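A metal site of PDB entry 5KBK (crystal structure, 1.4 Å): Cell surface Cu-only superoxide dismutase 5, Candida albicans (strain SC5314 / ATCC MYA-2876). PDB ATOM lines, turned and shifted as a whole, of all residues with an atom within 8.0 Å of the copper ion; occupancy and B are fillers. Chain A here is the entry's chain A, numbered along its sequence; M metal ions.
The backbone carbonyl oxygen of Glu 69 is in hydrogen-bond range of a ring nitrogen (ND1) of His 55 (2.8 Å). The backbone carbonyl oxygen of Asn 70 lies close to a ring nitrogen (ND1) of His 55. The backbone carbonyl oxygen (O) of Ser 127 lies within hydrogen-bond range of the backbone NH (N) of His 55, 2.8 Å away. The backbone NH of His 131 is in hydrogen-bond range of the backbone carbonyl oxygen of Pro 51 (2.9 Å). A ring nitrogen (ND1) of His 131 is in hydrogen-bond range of the backbone carbonyl oxygen (O) of Gly 135 (2.9 Å). The backbone carbonyl oxygen of His 53 is in hydrogen-bond range of the backbone NH of Val 129 (3.1 Å).
Residues that only touch the copper ion: His 71 (3.6 Å) and Val 129 (3.9 Å). The nearest printed residue that does not touch the copper ion is Tyr 52 (4.8 Å).
The copper ion is bound by NE2 of His 55 (2.0 Å). The copper ion is bound by a ring nitrogen (NE2) of His 131 (2.0 Å). The copper ion is bound by ND1 of His 53, at 2.0 Å.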
ATOM      1  N   PRO A  51     -22.418  -3.585  23.126  1.00  0.00           N
ATOM      2  CA  PRO A  51     -21.993  -4.992  23.108  1.00  0.00           C
ATOM      3  C   PRO A  51     -20.509  -5.116  23.454  1.00  0.00           C
ATOM      4  O   PRO A  51     -19.707  -4.204  23.214  1.00  0.00           O
ATOM      5  CB  PRO A  51     -22.262  -5.439  21.679  1.00  0.00           C
ATOM      6  CG  PRO A  51     -23.286  -4.436  21.137  1.00  0.00           C
ATOM      7  CD  PRO A  51     -22.900  -3.146  21.805  1.00  0.00           C
ATOM      8  N   TYR A  52     -20.166  -6.240  24.059  1.00  0.00           N
ATOM      9  CA  TYR A  52     -18.781  -6.553  24.371  1.00  0.00           C
ATOM     10  C   TYR A  52     -18.593  -8.070  24.291  1.00  0.00           C
ATOM     11  O   TYR A  52     -19.496  -8.838  24.652  1.00  0.00           O
ATOM     12  CB  TYR A  52     -18.313  -5.973  25.709  1.00  0.00           C
ATOM     13  CG  TYR A  52     -18.941  -6.574  26.949  1.00  0.00           C
ATOM     14  CD1 TYR A  52     -20.264  -6.316  27.278  1.00  0.00           C
ATOM     15  CD2 TYR A  52     -18.200  -7.356  27.828  1.00  0.00           C
ATOM     16  CE1 TYR A  52     -20.843  -6.863  28.410  1.00  0.00           C
ATOM     17  CE2 TYR A  52     -18.760  -7.887  28.979  1.00  0.00           C
ATOM     18  CZ  TYR A  52     -20.079  -7.639  29.266  1.00  0.00           C
ATOM     19  OH  TYR A  52     -20.635  -8.182  30.414  1.00  0.00           O
ATOM     20  N   HIS A  53     -17.456  -8.470  23.745  1.00  0.00           N
ATOM     21  CA  HIS A  53     -17.207  -9.872  23.429  1.00  0.00           C
ATOM     22  C   HIS A  53     -15.732 -10.179  23.580  1.00  0.00           C
ATOM     23  O   HIS A  53     -14.887  -9.284  23.485  1.00  0.00           O
ATOM     24  CB  HIS A  53     -17.590 -10.221  21.984  1.00  0.00           C
ATOM     25  CG  HIS A  53     -18.732  -9.440  21.442  1.00  0.00           C
ATOM     26  ND1 HIS A  53     -18.566  -8.285  20.714  1.00  0.00           N
ATOM     27  CD2 HIS A  53     -20.070  -9.674  21.481  1.00  0.00           C
ATOM     28  CE1 HIS A  53     -19.746  -7.820  20.351  1.00  0.00           C
ATOM     29  NE2 HIS A  53     -20.686  -8.646  20.801  1.00  0.00           N
ATOM     30  N   VAL A  54     -15.436 -11.451  23.777  1.00  0.00           N
ATOM     31  CA  VAL A  54     -14.091 -11.969  23.643  1.00  0.00           C
ATOM     32  C   VAL A  54     -13.788 -12.145  22.168  1.00  0.00           C
ATOM     33  O   VAL A  54     -14.577 -12.770  21.436  1.00  0.00           O
ATOM     34  CB  VAL A  54     -13.938 -13.321  24.381  1.00  0.00           C
ATOM     35  CG1 VAL A  54     -12.486 -13.780  24.280  1.00  0.00           C
ATOM     36  CG2 VAL A  54     -14.352 -13.211  25.817  1.00  0.00           C
ATOM     37  N   HIS A  55     -12.664 -11.602  21.728  1.00  0.00           N
ATOM     38  CA  HIS A  55     -12.213 -11.715  20.340  1.00  0.00           C
ATOM     39  C   HIS A  55     -11.002 -12.640  20.251  1.00  0.00           C
ATOM     40  O   HIS A  55     -10.387 -13.012  21.250  1.00  0.00           O
ATOM     41  CB  HIS A  55     -11.923 -10.339  19.742  1.00  0.00           C
ATOM     42  CG  HIS A  55     -13.158  -9.579  19.378  1.00  0.00           C
ATOM     43  ND1 HIS A  55     -13.470  -9.207  18.086  1.00  0.00           N
ATOM     44  CD2 HIS A  55     -14.186  -9.145  20.151  1.00  0.00           C
ATOM     45  CE1 HIS A  55     -14.632  -8.579  18.082  1.00  0.00           C
ATOM     46  NE2 HIS A  55     -15.087  -8.521  19.322  1.00  0.00           N
ATOM     47  N   CYS A  65      -8.045  -1.800  17.864  1.00  0.00           N
ATOM     48  CA  CYS A  65      -9.042  -2.807  18.231  1.00  0.00           C
ATOM     49  C   CYS A  65      -9.490  -3.643  17.050  1.00  0.00           C
ATOM     50  O   CYS A  65     -10.001  -4.758  17.240  1.00  0.00           O
ATOM     51  CB  CYS A  65     -10.226  -2.154  18.938  1.00  0.00           C
ATOM     52  SG  CYS A  65      -9.780  -1.324  20.490  1.00  0.00           S
ATOM     53  N   THR A  68      -7.819  -7.259  16.729  1.00  0.00           N
ATOM     54  CA  THR A  68      -8.267  -8.415  17.492  1.00  0.00           C
ATOM     55  C   THR A  68      -9.097  -9.374  16.630  1.00  0.00           C
ATOM     56  O   THR A  68      -9.429 -10.466  17.085  1.00  0.00           O
ATOM     57  CB  THR A  68      -9.095  -7.972  18.714  1.00  0.00           C
ATOM     58  OG1 THR A  68     -10.290  -7.323  18.275  1.00  0.00           O
ATOM     59  CG2 THR A  68      -8.308  -7.066  19.663  1.00  0.00           C
ATOM     60  N   GLU A  69      -9.445  -8.955  15.419  1.00  0.00           N
ATOM     61  CA  GLU A  69     -10.137  -9.763  14.414  1.00  0.00           C
ATOM     62  C   GLU A  69     -11.507 -10.198  14.956  1.00  0.00           C
ATOM     63  O   GLU A  69     -12.208  -9.383  15.568  1.00  0.00           O
ATOM     64  CB  GLU A  69      -9.259 -10.895  13.905  1.00  0.00           C
ATOM     65  CG  GLU A  69      -8.007 -10.450  13.207  1.00  0.00           C
ATOM     66  CD  GLU A  69      -7.148 -11.617  12.783  1.00  0.00           C
ATOM     67  OE1 GLU A  69      -7.628 -12.767  12.897  1.00  0.00           O
ATOM     68  OE2 GLU A  69      -5.999 -11.392  12.354  1.00  0.00           O
ATOM     69  N   ASN A  70     -11.889 -11.444  14.728  1.00  0.00           N
ATOM     70  CA  ASN A  70     -13.256 -11.892  14.839  1.00  0.00           C
ATOM     71  C   ASN A  70     -13.586 -12.322  16.264  1.00  0.00           C
ATOM     72  O   ASN A  70     -12.746 -12.353  17.160  1.00  0.00           O
ATOM     73  CB  ASN A  70     -13.510 -13.028  13.845  1.00  0.00           C
ATOM     74  CG  ASN A  70     -13.319 -12.604  12.409  1.00  0.00           C
ATOM     75  OD1 ASN A  70     -13.717 -11.507  12.016  1.00  0.00           O
ATOM     76  ND2 ASN A  70     -12.704 -13.464  11.604  1.00  0.00           N
ATOM     77  N   HIS A  71     -14.843 -12.686  16.474  1.00  0.00           N
ATOM     78  CA  HIS A  71     -15.290 -13.090  17.790  1.00  0.00           C
ATOM     79  C   HIS A  71     -14.787 -14.487  18.110  1.00  0.00           C
ATOM     80  O   HIS A  71     -14.707 -15.338  17.230  1.00  0.00           O
ATOM     81  CB  HIS A  71     -16.822 -13.065  17.838  1.00  0.00           C
ATOM     82  CG  HIS A  71     -17.404 -11.709  17.629  1.00  0.00           C
ATOM     83  ND1 HIS A  71     -18.474 -11.243  18.355  1.00  0.00           N
ATOM     84  CD2 HIS A  71     -17.063 -10.718  16.775  1.00  0.00           C
ATOM     85  CE1 HIS A  71     -18.762 -10.023  17.966  1.00  0.00           C
ATOM     86  NE2 HIS A  71     -17.926  -9.675  16.999  1.00  0.00           N
ATOM     87  N   PHE A  72     -14.453 -14.710  19.381  1.00  0.00           N
ATOM     88  CA  PHE A  72     -14.108 -16.059  19.837  1.00  0.00           C
ATOM     89  C   PHE A  72     -15.373 -16.905  19.858  1.00  0.00           C
ATOM     90  O   PHE A  72     -16.272 -16.682  20.671  1.00  0.00           O
ATOM     91  CB  PHE A  72     -13.482 -15.983  21.229  1.00  0.00           C
ATOM     92  CG  PHE A  72     -13.098 -17.329  21.790  1.00  0.00           C
ATOM     93  CD1 PHE A  72     -12.196 -18.137  21.136  1.00  0.00           C
ATOM     94  CD2 PHE A  72     -13.625 -17.762  22.989  1.00  0.00           C
ATOM     95  CE1 PHE A  72     -11.833 -19.367  21.656  1.00  0.00           C
ATOM     96  CE2 PHE A  72     -13.264 -18.968  23.533  1.00  0.00           C
ATOM     97  CZ  PHE A  72     -12.362 -19.780  22.865  1.00  0.00           C
ATOM     98  N   GLY A  90     -17.680 -16.436  23.655  1.00  0.00           N
ATOM     99  CA  GLY A  90     -17.229 -15.132  24.087  1.00  0.00           C
ATOM    100  C   GLY A  90     -18.242 -14.031  23.953  1.00  0.00           C
ATOM    101  O   GLY A  90     -17.893 -12.868  24.180  1.00  0.00           O
ATOM    102  N   ASP A  91     -19.499 -14.346  23.609  1.00  0.00           N
ATOM    103  CA  ASP A  91     -20.526 -13.328  23.448  1.00  0.00           C
ATOM    104  C   ASP A  91     -21.120 -13.016  24.819  1.00  0.00           C
ATOM    105  O   ASP A  91     -22.245 -13.395  25.167  1.00  0.00           O
ATOM    106  CB  ASP A  91     -21.579 -13.766  22.437  1.00  0.00           C
ATOM    107  CG  ASP A  91     -22.622 -12.702  22.214  1.00  0.00           C
ATOM    108  OD1 ASP A  91     -22.431 -11.546  22.676  1.00  0.00           O
ATOM    109  OD2 ASP A  91     -23.649 -13.017  21.570  1.00  0.00           O
ATOM    110  N   SER A 127      -8.727 -11.294  23.884  1.00  0.00           N
ATOM    111  CA  SER A 127      -8.979  -9.880  24.089  1.00  0.00           C
ATOM    112  C   SER A 127     -10.470  -9.661  24.281  1.00  0.00           C
ATOM    113  O   SER A 127     -11.283 -10.528  23.945  1.00  0.00           O
ATOM    114  CB  SER A 127      -8.526  -9.057  22.889  1.00  0.00           C
ATOM    115  OG  SER A 127      -9.143  -9.516  21.694  1.00  0.00           O
ATOM    116  N   ILE A 128     -10.817  -8.511  24.852  1.00  0.00           N
ATOM    117  CA  ILE A 128     -12.198  -8.061  24.940  1.00  0.00           C
ATOM    118  C   ILE A 128     -12.307  -6.766  24.159  1.00  0.00           C
ATOM    119  O   ILE A 128     -11.462  -5.880  24.305  1.00  0.00           O
ATOM    120  CB  ILE A 128     -12.643  -7.882  26.394  1.00  0.00           C
ATOM    121  CG1 ILE A 128     -12.594  -9.232  27.109  1.00  0.00           C
ATOM    122  CG2 ILE A 128     -14.055  -7.291  26.450  1.00  0.00           C
ATOM    123  CD1 ILE A 128     -12.843  -9.176  28.577  1.00  0.00           C
ATOM    124  N   VAL A 129     -13.341  -6.653  23.331  1.00  0.00           N
ATOM    125  CA  VAL A 129     -13.676  -5.429  22.619  1.00  0.00           C
ATOM    126  C   VAL A 129     -15.025  -4.926  23.104  1.00  0.00           C
ATOM    127  O   VAL A 129     -15.978  -5.703  23.223  1.00  0.00           O
ATOM    128  CB  VAL A 129     -13.712  -5.682  21.089  1.00  0.00           C
ATOM    129  CG1 VAL A 129     -14.102  -4.421  20.350  1.00  0.00           C
ATOM    130  CG2 VAL A 129     -12.384  -6.178  20.608  1.00  0.00           C
ATOM    131  N   ILE A 130     -15.118  -3.617  23.322  1.00  0.00           N
ATOM    132  CA  ILE A 130     -16.366  -2.925  23.624  1.00  0.00           C
ATOM    133  C   ILE A 130     -16.738  -2.121  22.388  1.00  0.00           C
ATOM    134  O   ILE A 130     -15.919  -1.352  21.860  1.00  0.00           O
ATOM    135  CB  ILE A 130     -16.217  -2.005  24.850  1.00  0.00           C
ATOM    136  CG1 ILE A 130     -15.801  -2.795  26.094  1.00  0.00           C
ATOM    137  CG2 ILE A 130     -17.516  -1.217  25.120  1.00  0.00           C
ATOM    138  CD1 ILE A 130     -15.413  -1.928  27.307  1.00  0.00           C
ATOM    139  N   HIS A 131     -17.976  -2.309  21.918  1.00  0.00           N
ATOM    140  CA  HIS A 131     -18.472  -1.696  20.697  1.00  0.00           C
ATOM    141  C   HIS A 131     -19.531  -0.653  21.021  1.00  0.00           C
ATOM    142  O   HIS A 131     -20.278  -0.782  21.993  1.00  0.00           O
ATOM    143  CB  HIS A 131     -19.172  -2.729  19.797  1.00  0.00           C
ATOM    144  CG  HIS A 131     -18.313  -3.898  19.425  1.00  0.00           C
ATOM    145  ND1 HIS A 131     -17.802  -4.062  18.161  1.00  0.00           N
ATOM    146  CD2 HIS A 131     -17.948  -4.996  20.120  1.00  0.00           C
ATOM    147  CE1 HIS A 131     -17.125  -5.192  18.099  1.00  0.00           C
ATOM    148  NE2 HIS A 131     -17.220  -5.795  19.276  1.00  0.00           N
ATOM    149  N   GLY A 135     -21.639  -1.041  16.163  1.00  0.00           N
ATOM    150  CA  GLY A 135     -20.574  -1.980  15.913  1.00  0.00           C
ATOM    151  C   GLY A 135     -19.184  -1.391  15.971  1.00  0.00           C
ATOM    152  O   GLY A 135     -18.223  -2.148  16.079  1.00  0.00           O
ATOM    153  N   ARG A 137     -15.736  -0.247  17.070  1.00  0.00           N
ATOM    154  CA  ARG A 137     -14.944  -0.691  18.215  1.00  0.00           C
ATOM    155  C   ARG A 137     -14.400   0.529  18.955  1.00  0.00           C
ATOM    156  O   ARG A 137     -13.675   1.344  18.381  1.00  0.00           O
ATOM    157  CB  ARG A 137     -13.823  -1.610  17.726  1.00  0.00           C
ATOM    158  CG  ARG A 137     -14.344  -2.806  16.961  1.00  0.00           C
ATOM    159  CD  ARG A 137     -13.278  -3.799  16.541  1.00  0.00           C
ATOM    160  NE  ARG A 137     -13.923  -4.906  15.827  1.00  0.00           N
ATOM    161  CZ  ARG A 137     -13.380  -6.103  15.609  1.00  0.00           C
ATOM    162  NH1 ARG A 137     -12.162  -6.399  16.048  1.00  0.00           N
ATOM    163  NH2 ARG A 137     -14.095  -7.029  14.939  1.00  0.00           N
ATOM    164  N   ASN A 139     -13.013   0.570  22.549  1.00  0.00           N
ATOM    165  CA  ASN A 139     -11.819   0.279  23.325  1.00  0.00           C
ATOM    166  C   ASN A 139     -11.706  -1.236  23.420  1.00  0.00           C
ATOM    167  O   ASN A 139     -12.656  -1.976  23.148  1.00  0.00           O
ATOM    168  CB  ASN A 139     -11.862   0.973  24.699  1.00  0.00           C
ATOM    169  CG  ASN A 139     -10.467   1.200  25.311  1.00  0.00           C
ATOM    170  OD1 ASN A 139      -9.459   0.658  24.842  1.00  0.00           O
ATOM    171  ND2 ASN A 139     -10.420   1.977  26.385  1.00  0.00           N
HETATM  172 CU    CU M   1     -16.812  -7.713  19.835  1.00  0.00          CU
